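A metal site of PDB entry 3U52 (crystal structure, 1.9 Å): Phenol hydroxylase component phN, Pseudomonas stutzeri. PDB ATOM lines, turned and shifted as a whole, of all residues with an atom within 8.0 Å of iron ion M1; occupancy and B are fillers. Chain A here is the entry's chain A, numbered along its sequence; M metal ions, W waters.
The side-chain amide nitrogen of Gln 134 sits close to a ring nitrogen (ND1) of His 236, at 3.4 Å.
A ring nitrogen (NE2) of His 236 sits at hydrogen-bond distance from the side-chain carboxylate (OD2) of Asp 137.
N of Glu 199 lies within hydrogen-bond range of O of Ile 194, at 2.7 Å.
NE2 of Gln 134 is in hydrogen-bond range of OE1 of Glu 138 (2.9 Å).
The side-chain carboxylate (OE1) of Glu 199 lies close to the side-chain amide nitrogen (NE2) of Gln 134 (2.8 Å).
Residues that only touch iron ion M1: Glu 138 and Gln 134.
Five residues have an atom within 4 Å of iron ion M1: Gln 134, Glu 138, Glu 199, Glu 233 and His 236.
Iron ion M1 is bound by OE2 of Glu 233, OE1 of Glu 199, ND1 of His 236 and OE1 of Glu 233.
Iron ion M1 has four donor atoms within binding distance.
Slightly farther from iron ion M1 lies water W1 (2.8 Å).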
ATOM      1  N   GLU A 108     -22.780 -11.970 -19.116  1.00  0.00           N
ATOM      2  CA  GLU A 108     -23.499 -12.360 -17.898  1.00  0.00           C
ATOM      3  C   GLU A 108     -22.434 -13.114 -17.087  1.00  0.00           C
ATOM      4  O   GLU A 108     -22.311 -12.946 -15.878  1.00  0.00           O
ATOM      5  CB  GLU A 108     -24.660 -13.323 -18.199  1.00  0.00           C
ATOM      6  CG  GLU A 108     -25.823 -12.777 -19.095  1.00  0.00           C
ATOM      7  CD  GLU A 108     -26.754 -11.881 -18.316  1.00  0.00           C
ATOM      8  OE1 GLU A 108     -27.858 -11.578 -18.798  1.00  0.00           O
ATOM      9  OE2 GLU A 108     -26.369 -11.472 -17.225  1.00  0.00           O
ATOM     10  N   ALA A 111     -19.879 -11.057 -15.545  1.00  0.00           N
ATOM     11  CA  ALA A 111     -20.404 -10.299 -14.402  1.00  0.00           C
ATOM     12  C   ALA A 111     -20.409 -11.221 -13.176  1.00  0.00           C
ATOM     13  O   ALA A 111     -20.120 -10.789 -12.035  1.00  0.00           O
ATOM     14  CB  ALA A 111     -21.747  -9.768 -14.702  1.00  0.00           C
ATOM     15  N   TYR A 115     -18.490  -9.777 -10.031  1.00  0.00           N
ATOM     16  CA  TYR A 115     -19.206  -9.591  -8.778  1.00  0.00           C
ATOM     17  C   TYR A 115     -18.718 -10.542  -7.670  1.00  0.00           C
ATOM     18  O   TYR A 115     -18.703 -10.155  -6.491  1.00  0.00           O
ATOM     19  CB  TYR A 115     -20.719  -9.739  -8.972  1.00  0.00           C
ATOM     20  CG  TYR A 115     -21.369  -8.451  -9.445  1.00  0.00           C
ATOM     21  CD1 TYR A 115     -21.684  -8.281 -10.804  1.00  0.00           C
ATOM     22  CD2 TYR A 115     -21.587  -7.387  -8.558  1.00  0.00           C
ATOM     23  CE1 TYR A 115     -22.234  -7.100 -11.257  1.00  0.00           C
ATOM     24  CE2 TYR A 115     -22.158  -6.179  -9.020  1.00  0.00           C
ATOM     25  CZ  TYR A 115     -22.464  -6.047 -10.364  1.00  0.00           C
ATOM     26  OH  TYR A 115     -23.040  -4.903 -10.820  1.00  0.00           O
ATOM     27  N   GLN A 134     -25.847 -10.816  -6.167  1.00  0.00           N
ATOM     28  CA  GLN A 134     -25.793 -10.430  -7.581  1.00  0.00           C
ATOM     29  C   GLN A 134     -24.913 -11.403  -8.402  1.00  0.00           C
ATOM     30  O   GLN A 134     -25.321 -11.898  -9.445  1.00  0.00           O
ATOM     31  CB  GLN A 134     -25.356  -8.968  -7.748  1.00  0.00           C
ATOM     32  CG  GLN A 134     -25.149  -8.634  -9.184  1.00  0.00           C
ATOM     33  CD  GLN A 134     -25.876  -7.419  -9.643  1.00  0.00           C
ATOM     34  OE1 GLN A 134     -26.348  -6.606  -8.833  1.00  0.00           O
ATOM     35  NE2 GLN A 134     -26.008  -7.283 -10.967  1.00  0.00           N
ATOM     36  N   ASP A 137     -26.853 -14.599  -9.081  1.00  0.00           N
ATOM     37  CA  ASP A 137     -27.867 -14.304 -10.115  1.00  0.00           C
ATOM     38  C   ASP A 137     -27.295 -14.225 -11.521  1.00  0.00           C
ATOM     39  O   ASP A 137     -27.943 -14.647 -12.496  1.00  0.00           O
ATOM     40  CB  ASP A 137     -28.606 -12.970  -9.841  1.00  0.00           C
ATOM     41  CG  ASP A 137     -29.405 -12.950  -8.553  1.00  0.00           C
ATOM     42  OD1 ASP A 137     -29.776 -13.976  -7.928  1.00  0.00           O
ATOM     43  OD2 ASP A 137     -29.649 -11.795  -8.123  1.00  0.00           O
ATOM     44  N   GLU A 138     -26.120 -13.611 -11.693  1.00  0.00           N
ATOM     45  CA  GLU A 138     -25.498 -13.535 -13.039  1.00  0.00           C
ATOM     46  C   GLU A 138     -25.070 -14.915 -13.527  1.00  0.00           C
ATOM     47  O   GLU A 138     -25.163 -15.201 -14.724  1.00  0.00           O
ATOM     48  CB  GLU A 138     -24.291 -12.609 -13.051  1.00  0.00           C
ATOM     49  CG  GLU A 138     -24.637 -11.244 -12.465  1.00  0.00           C
ATOM     50  CD  GLU A 138     -25.572 -10.447 -13.384  1.00  0.00           C
ATOM     51  OE1 GLU A 138     -25.911  -9.316 -13.032  1.00  0.00           O
ATOM     52  OE2 GLU A 138     -25.978 -10.945 -14.461  1.00  0.00           O
ATOM     53  N   HIS A 141     -28.102 -16.307 -14.868  1.00  0.00           N
ATOM     54  CA  HIS A 141     -28.486 -15.685 -16.144  1.00  0.00           C
ATOM     55  C   HIS A 141     -27.683 -16.276 -17.264  1.00  0.00           C
ATOM     56  O   HIS A 141     -28.212 -16.612 -18.311  1.00  0.00           O
ATOM     57  CB  HIS A 141     -28.309 -14.145 -16.065  1.00  0.00           C
ATOM     58  CG  HIS A 141     -29.329 -13.482 -15.188  1.00  0.00           C
ATOM     59  ND1 HIS A 141     -29.289 -12.144 -14.871  1.00  0.00           N
ATOM     60  CD2 HIS A 141     -30.422 -13.980 -14.541  1.00  0.00           C
ATOM     61  CE1 HIS A 141     -30.295 -11.837 -14.077  1.00  0.00           C
ATOM     62  NE2 HIS A 141     -31.010 -12.932 -13.880  1.00  0.00           N
ATOM     63  N   ILE A 194     -20.878  -0.999 -13.665  1.00  0.00           N
ATOM     64  CA  ILE A 194     -21.781  -2.119 -13.904  1.00  0.00           C
ATOM     65  C   ILE A 194     -23.108  -2.010 -13.126  1.00  0.00           C
ATOM     66  O   ILE A 194     -24.201  -2.101 -13.717  1.00  0.00           O
ATOM     67  CB  ILE A 194     -21.053  -3.535 -13.765  1.00  0.00           C
ATOM     68  CG1 ILE A 194     -19.765  -3.595 -14.630  1.00  0.00           C
ATOM     69  CG2 ILE A 194     -21.993  -4.692 -14.142  1.00  0.00           C
ATOM     70  CD1 ILE A 194     -19.898  -3.264 -16.193  1.00  0.00           C
ATOM     71  N   PHE A 198     -24.737   0.450 -15.963  1.00  0.00           N
ATOM     72  CA  PHE A 198     -25.267  -0.641 -16.773  1.00  0.00           C
ATOM     73  C   PHE A 198     -26.611  -1.042 -16.165  1.00  0.00           C
ATOM     74  O   PHE A 198     -27.667  -0.904 -16.815  1.00  0.00           O
ATOM     75  CB  PHE A 198     -24.260  -1.807 -16.654  1.00  0.00           C
ATOM     76  CG  PHE A 198     -24.155  -2.744 -17.842  1.00  0.00           C
ATOM     77  CD1 PHE A 198     -24.472  -2.377 -19.132  1.00  0.00           C
ATOM     78  CD2 PHE A 198     -23.595  -4.021 -17.653  1.00  0.00           C
ATOM     79  CE1 PHE A 198     -24.314  -3.334 -20.188  1.00  0.00           C
ATOM     80  CE2 PHE A 198     -23.406  -4.929 -18.723  1.00  0.00           C
ATOM     81  CZ  PHE A 198     -23.774  -4.595 -19.961  1.00  0.00           C
ATOM     82  N   GLU A 199     -26.594  -1.488 -14.900  1.00  0.00           N
ATOM     83  CA  GLU A 199     -27.772  -2.140 -14.266  1.00  0.00           C
ATOM     84  C   GLU A 199     -28.847  -1.220 -13.804  1.00  0.00           C
ATOM     85  O   GLU A 199     -29.925  -1.689 -13.496  1.00  0.00           O
ATOM     86  CB  GLU A 199     -27.387  -2.958 -13.042  1.00  0.00           C
ATOM     87  CG  GLU A 199     -26.514  -4.155 -13.350  1.00  0.00           C
ATOM     88  CD  GLU A 199     -27.334  -5.307 -13.908  1.00  0.00           C
ATOM     89  OE1 GLU A 199     -27.379  -6.381 -13.286  1.00  0.00           O
ATOM     90  OE2 GLU A 199     -27.944  -5.128 -14.982  1.00  0.00           O
ATOM     91  N   TYR A 200     -28.569   0.066 -13.685  1.00  0.00           N
ATOM     92  CA  TYR A 200     -29.584   0.980 -13.260  1.00  0.00           C
ATOM     93  C   TYR A 200     -29.935   1.968 -14.364  1.00  0.00           C
ATOM     94  O   TYR A 200     -31.095   2.033 -14.793  1.00  0.00           O
ATOM     95  CB  TYR A 200     -29.196   1.692 -11.953  1.00  0.00           C
ATOM     96  CG  TYR A 200     -30.319   2.540 -11.451  1.00  0.00           C
ATOM     97  CD1 TYR A 200     -30.316   3.903 -11.632  1.00  0.00           C
ATOM     98  CD2 TYR A 200     -31.428   1.963 -10.845  1.00  0.00           C
ATOM     99  CE1 TYR A 200     -31.416   4.694 -11.200  1.00  0.00           C
ATOM    100  CE2 TYR A 200     -32.491   2.699 -10.423  1.00  0.00           C
ATOM    101  CZ  TYR A 200     -32.493   4.078 -10.599  1.00  0.00           C
ATOM    102  OH  TYR A 200     -33.582   4.826 -10.128  1.00  0.00           O
ATOM    103  N   THR A 203     -29.972  -0.186 -18.224  1.00  0.00           N
ATOM    104  CA  THR A 203     -30.564  -1.542 -18.201  1.00  0.00           C
ATOM    105  C   THR A 203     -31.753  -1.795 -19.147  1.00  0.00           C
ATOM    106  O   THR A 203     -31.780  -2.773 -19.903  1.00  0.00           O
ATOM    107  CB  THR A 203     -30.929  -2.000 -16.755  1.00  0.00           C
ATOM    108  OG1 THR A 203     -31.281  -3.371 -16.812  1.00  0.00           O
ATOM    109  CG2 THR A 203     -32.091  -1.185 -16.143  1.00  0.00           C
ATOM    110  N   PHE A 207     -32.476  -4.730 -21.978  1.00  0.00           N
ATOM    111  CA  PHE A 207     -33.504  -5.709 -21.598  1.00  0.00           C
ATOM    112  C   PHE A 207     -34.791  -5.598 -22.385  1.00  0.00           C
ATOM    113  O   PHE A 207     -35.278  -6.599 -22.923  1.00  0.00           O
ATOM    114  CB  PHE A 207     -33.816  -5.529 -20.092  1.00  0.00           C
ATOM    115  CG  PHE A 207     -34.630  -6.652 -19.474  1.00  0.00           C
ATOM    116  CD1 PHE A 207     -36.025  -6.598 -19.472  1.00  0.00           C
ATOM    117  CD2 PHE A 207     -33.994  -7.734 -18.858  1.00  0.00           C
ATOM    118  CE1 PHE A 207     -36.765  -7.635 -18.898  1.00  0.00           C
ATOM    119  CE2 PHE A 207     -34.720  -8.768 -18.284  1.00  0.00           C
ATOM    120  CZ  PHE A 207     -36.104  -8.726 -18.298  1.00  0.00           C
ATOM    121  N   ALA A 229     -36.321 -13.282 -15.189  1.00  0.00           N
ATOM    122  CA  ALA A 229     -35.255 -12.422 -14.750  1.00  0.00           C
ATOM    123  C   ALA A 229     -35.736 -11.100 -14.161  1.00  0.00           C
ATOM    124  O   ALA A 229     -34.942 -10.422 -13.533  1.00  0.00           O
ATOM    125  CB  ALA A 229     -34.311 -12.171 -15.893  1.00  0.00           C
ATOM    126  N   ASP A 232     -35.138 -10.594 -10.422  1.00  0.00           N
ATOM    127  CA  ASP A 232     -33.706 -10.502 -10.209  1.00  0.00           C
ATOM    128  C   ASP A 232     -33.292  -9.056 -10.481  1.00  0.00           C
ATOM    129  O   ASP A 232     -32.625  -8.467  -9.660  1.00  0.00           O
ATOM    130  CB  ASP A 232     -32.900 -11.406 -11.162  1.00  0.00           C
ATOM    131  CG  ASP A 232     -33.116 -12.909 -10.916  1.00  0.00           C
ATOM    132  OD1 ASP A 232     -33.589 -13.336  -9.850  1.00  0.00           O
ATOM    133  OD2 ASP A 232     -32.747 -13.680 -11.832  1.00  0.00           O
ATOM    134  N   GLU A 233     -33.705  -8.503 -11.613  1.00  0.00           N
ATOM    135  CA  GLU A 233     -33.259  -7.165 -12.030  1.00  0.00           C
ATOM    136  C   GLU A 233     -33.761  -6.074 -11.161  1.00  0.00           C
ATOM    137  O   GLU A 233     -33.093  -5.053 -11.045  1.00  0.00           O
ATOM    138  CB  GLU A 233     -33.610  -6.817 -13.501  1.00  0.00           C
ATOM    139  CG  GLU A 233     -32.918  -7.722 -14.517  1.00  0.00           C
ATOM    140  CD  GLU A 233     -31.416  -7.934 -14.268  1.00  0.00           C
ATOM    141  OE1 GLU A 233     -30.998  -9.099 -14.282  1.00  0.00           O
ATOM    142  OE2 GLU A 233     -30.629  -6.990 -14.041  1.00  0.00           O
ATOM    143  N   ALA A 234     -34.933  -6.264 -10.545  1.00  0.00           N
ATOM    144  CA  ALA A 234     -35.398  -5.362  -9.500  1.00  0.00           C
ATOM    145  C   ALA A 234     -34.386  -5.236  -8.359  1.00  0.00           C
ATOM    146  O   ALA A 234     -34.158  -4.135  -7.854  1.00  0.00           O
ATOM    147  CB  ALA A 234     -36.758  -5.806  -8.952  1.00  0.00           C
ATOM    148  N   ARG A 235     -33.790  -6.342  -7.911  1.00  0.00           N
ATOM    149  CA  ARG A 235     -32.762  -6.237  -6.889  1.00  0.00           C
ATOM    150  C   ARG A 235     -31.502  -5.544  -7.452  1.00  0.00           C
ATOM    151  O   ARG A 235     -30.800  -4.797  -6.754  1.00  0.00           O
ATOM    152  CB  ARG A 235     -32.375  -7.642  -6.402  1.00  0.00           C
ATOM    153  CG  ARG A 235     -33.477  -8.372  -5.647  1.00  0.00           C
ATOM    154  CD  ARG A 235     -32.866  -9.540  -4.891  1.00  0.00           C
ATOM    155  NE  ARG A 235     -32.267 -10.549  -5.787  1.00  0.00           N
ATOM    156  CZ  ARG A 235     -32.974 -11.515  -6.379  1.00  0.00           C
ATOM    157  NH1 ARG A 235     -34.285 -11.609  -6.168  1.00  0.00           N
ATOM    158  NH2 ARG A 235     -32.396 -12.400  -7.159  1.00  0.00           N
ATOM    159  N   HIS A 236     -31.162  -5.860  -8.707  1.00  0.00           N
ATOM    160  CA  HIS A 236     -29.912  -5.350  -9.290  1.00  0.00           C
ATOM    161  C   HIS A 236     -29.993  -3.833  -9.488  1.00  0.00           C
ATOM    162  O   HIS A 236     -29.013  -3.125  -9.242  1.00  0.00           O
ATOM    163  CB  HIS A 236     -29.570  -6.090 -10.593  1.00  0.00           C
ATOM    164  CG  HIS A 236     -29.386  -7.556 -10.395  1.00  0.00           C
ATOM    165  ND1 HIS A 236     -29.182  -8.436 -11.437  1.00  0.00           N
ATOM    166  CD2 HIS A 236     -29.415  -8.317  -9.272  1.00  0.00           C
ATOM    167  CE1 HIS A 236     -29.052  -9.667 -10.961  1.00  0.00           C
ATOM    168  NE2 HIS A 236     -29.227  -9.628  -9.649  1.00  0.00           N
ATOM    169  N   MET A 237     -31.154  -3.339  -9.908  1.00  0.00           N
ATOM    170  CA  MET A 237     -31.358  -1.890 -10.014  1.00  0.00           C
ATOM    171  C   MET A 237     -31.288  -1.167  -8.671  1.00  0.00           C
ATOM    172  O   MET A 237     -30.752  -0.083  -8.602  1.00  0.00           O
ATOM    173  CB  MET A 237     -32.722  -1.555 -10.650  1.00  0.00           C
ATOM    174  CG  MET A 237     -32.873  -2.104 -12.036  1.00  0.00           C
ATOM    175  SD  MET A 237     -34.513  -1.738 -12.718  1.00  0.00           S
ATOM    176  CE  MET A 237     -34.254  -0.056 -13.280  1.00  0.00           C
HETATM  177 FE    FE M   1     -28.832  -7.897 -13.703  1.00  0.00          FE
HETATM  178 FE    FE M   2     -27.738 -10.518 -15.654  1.00  0.00          FE
HETATM  179  O   HOH W   1     -28.976  -6.932 -16.368  1.00  0.00           O
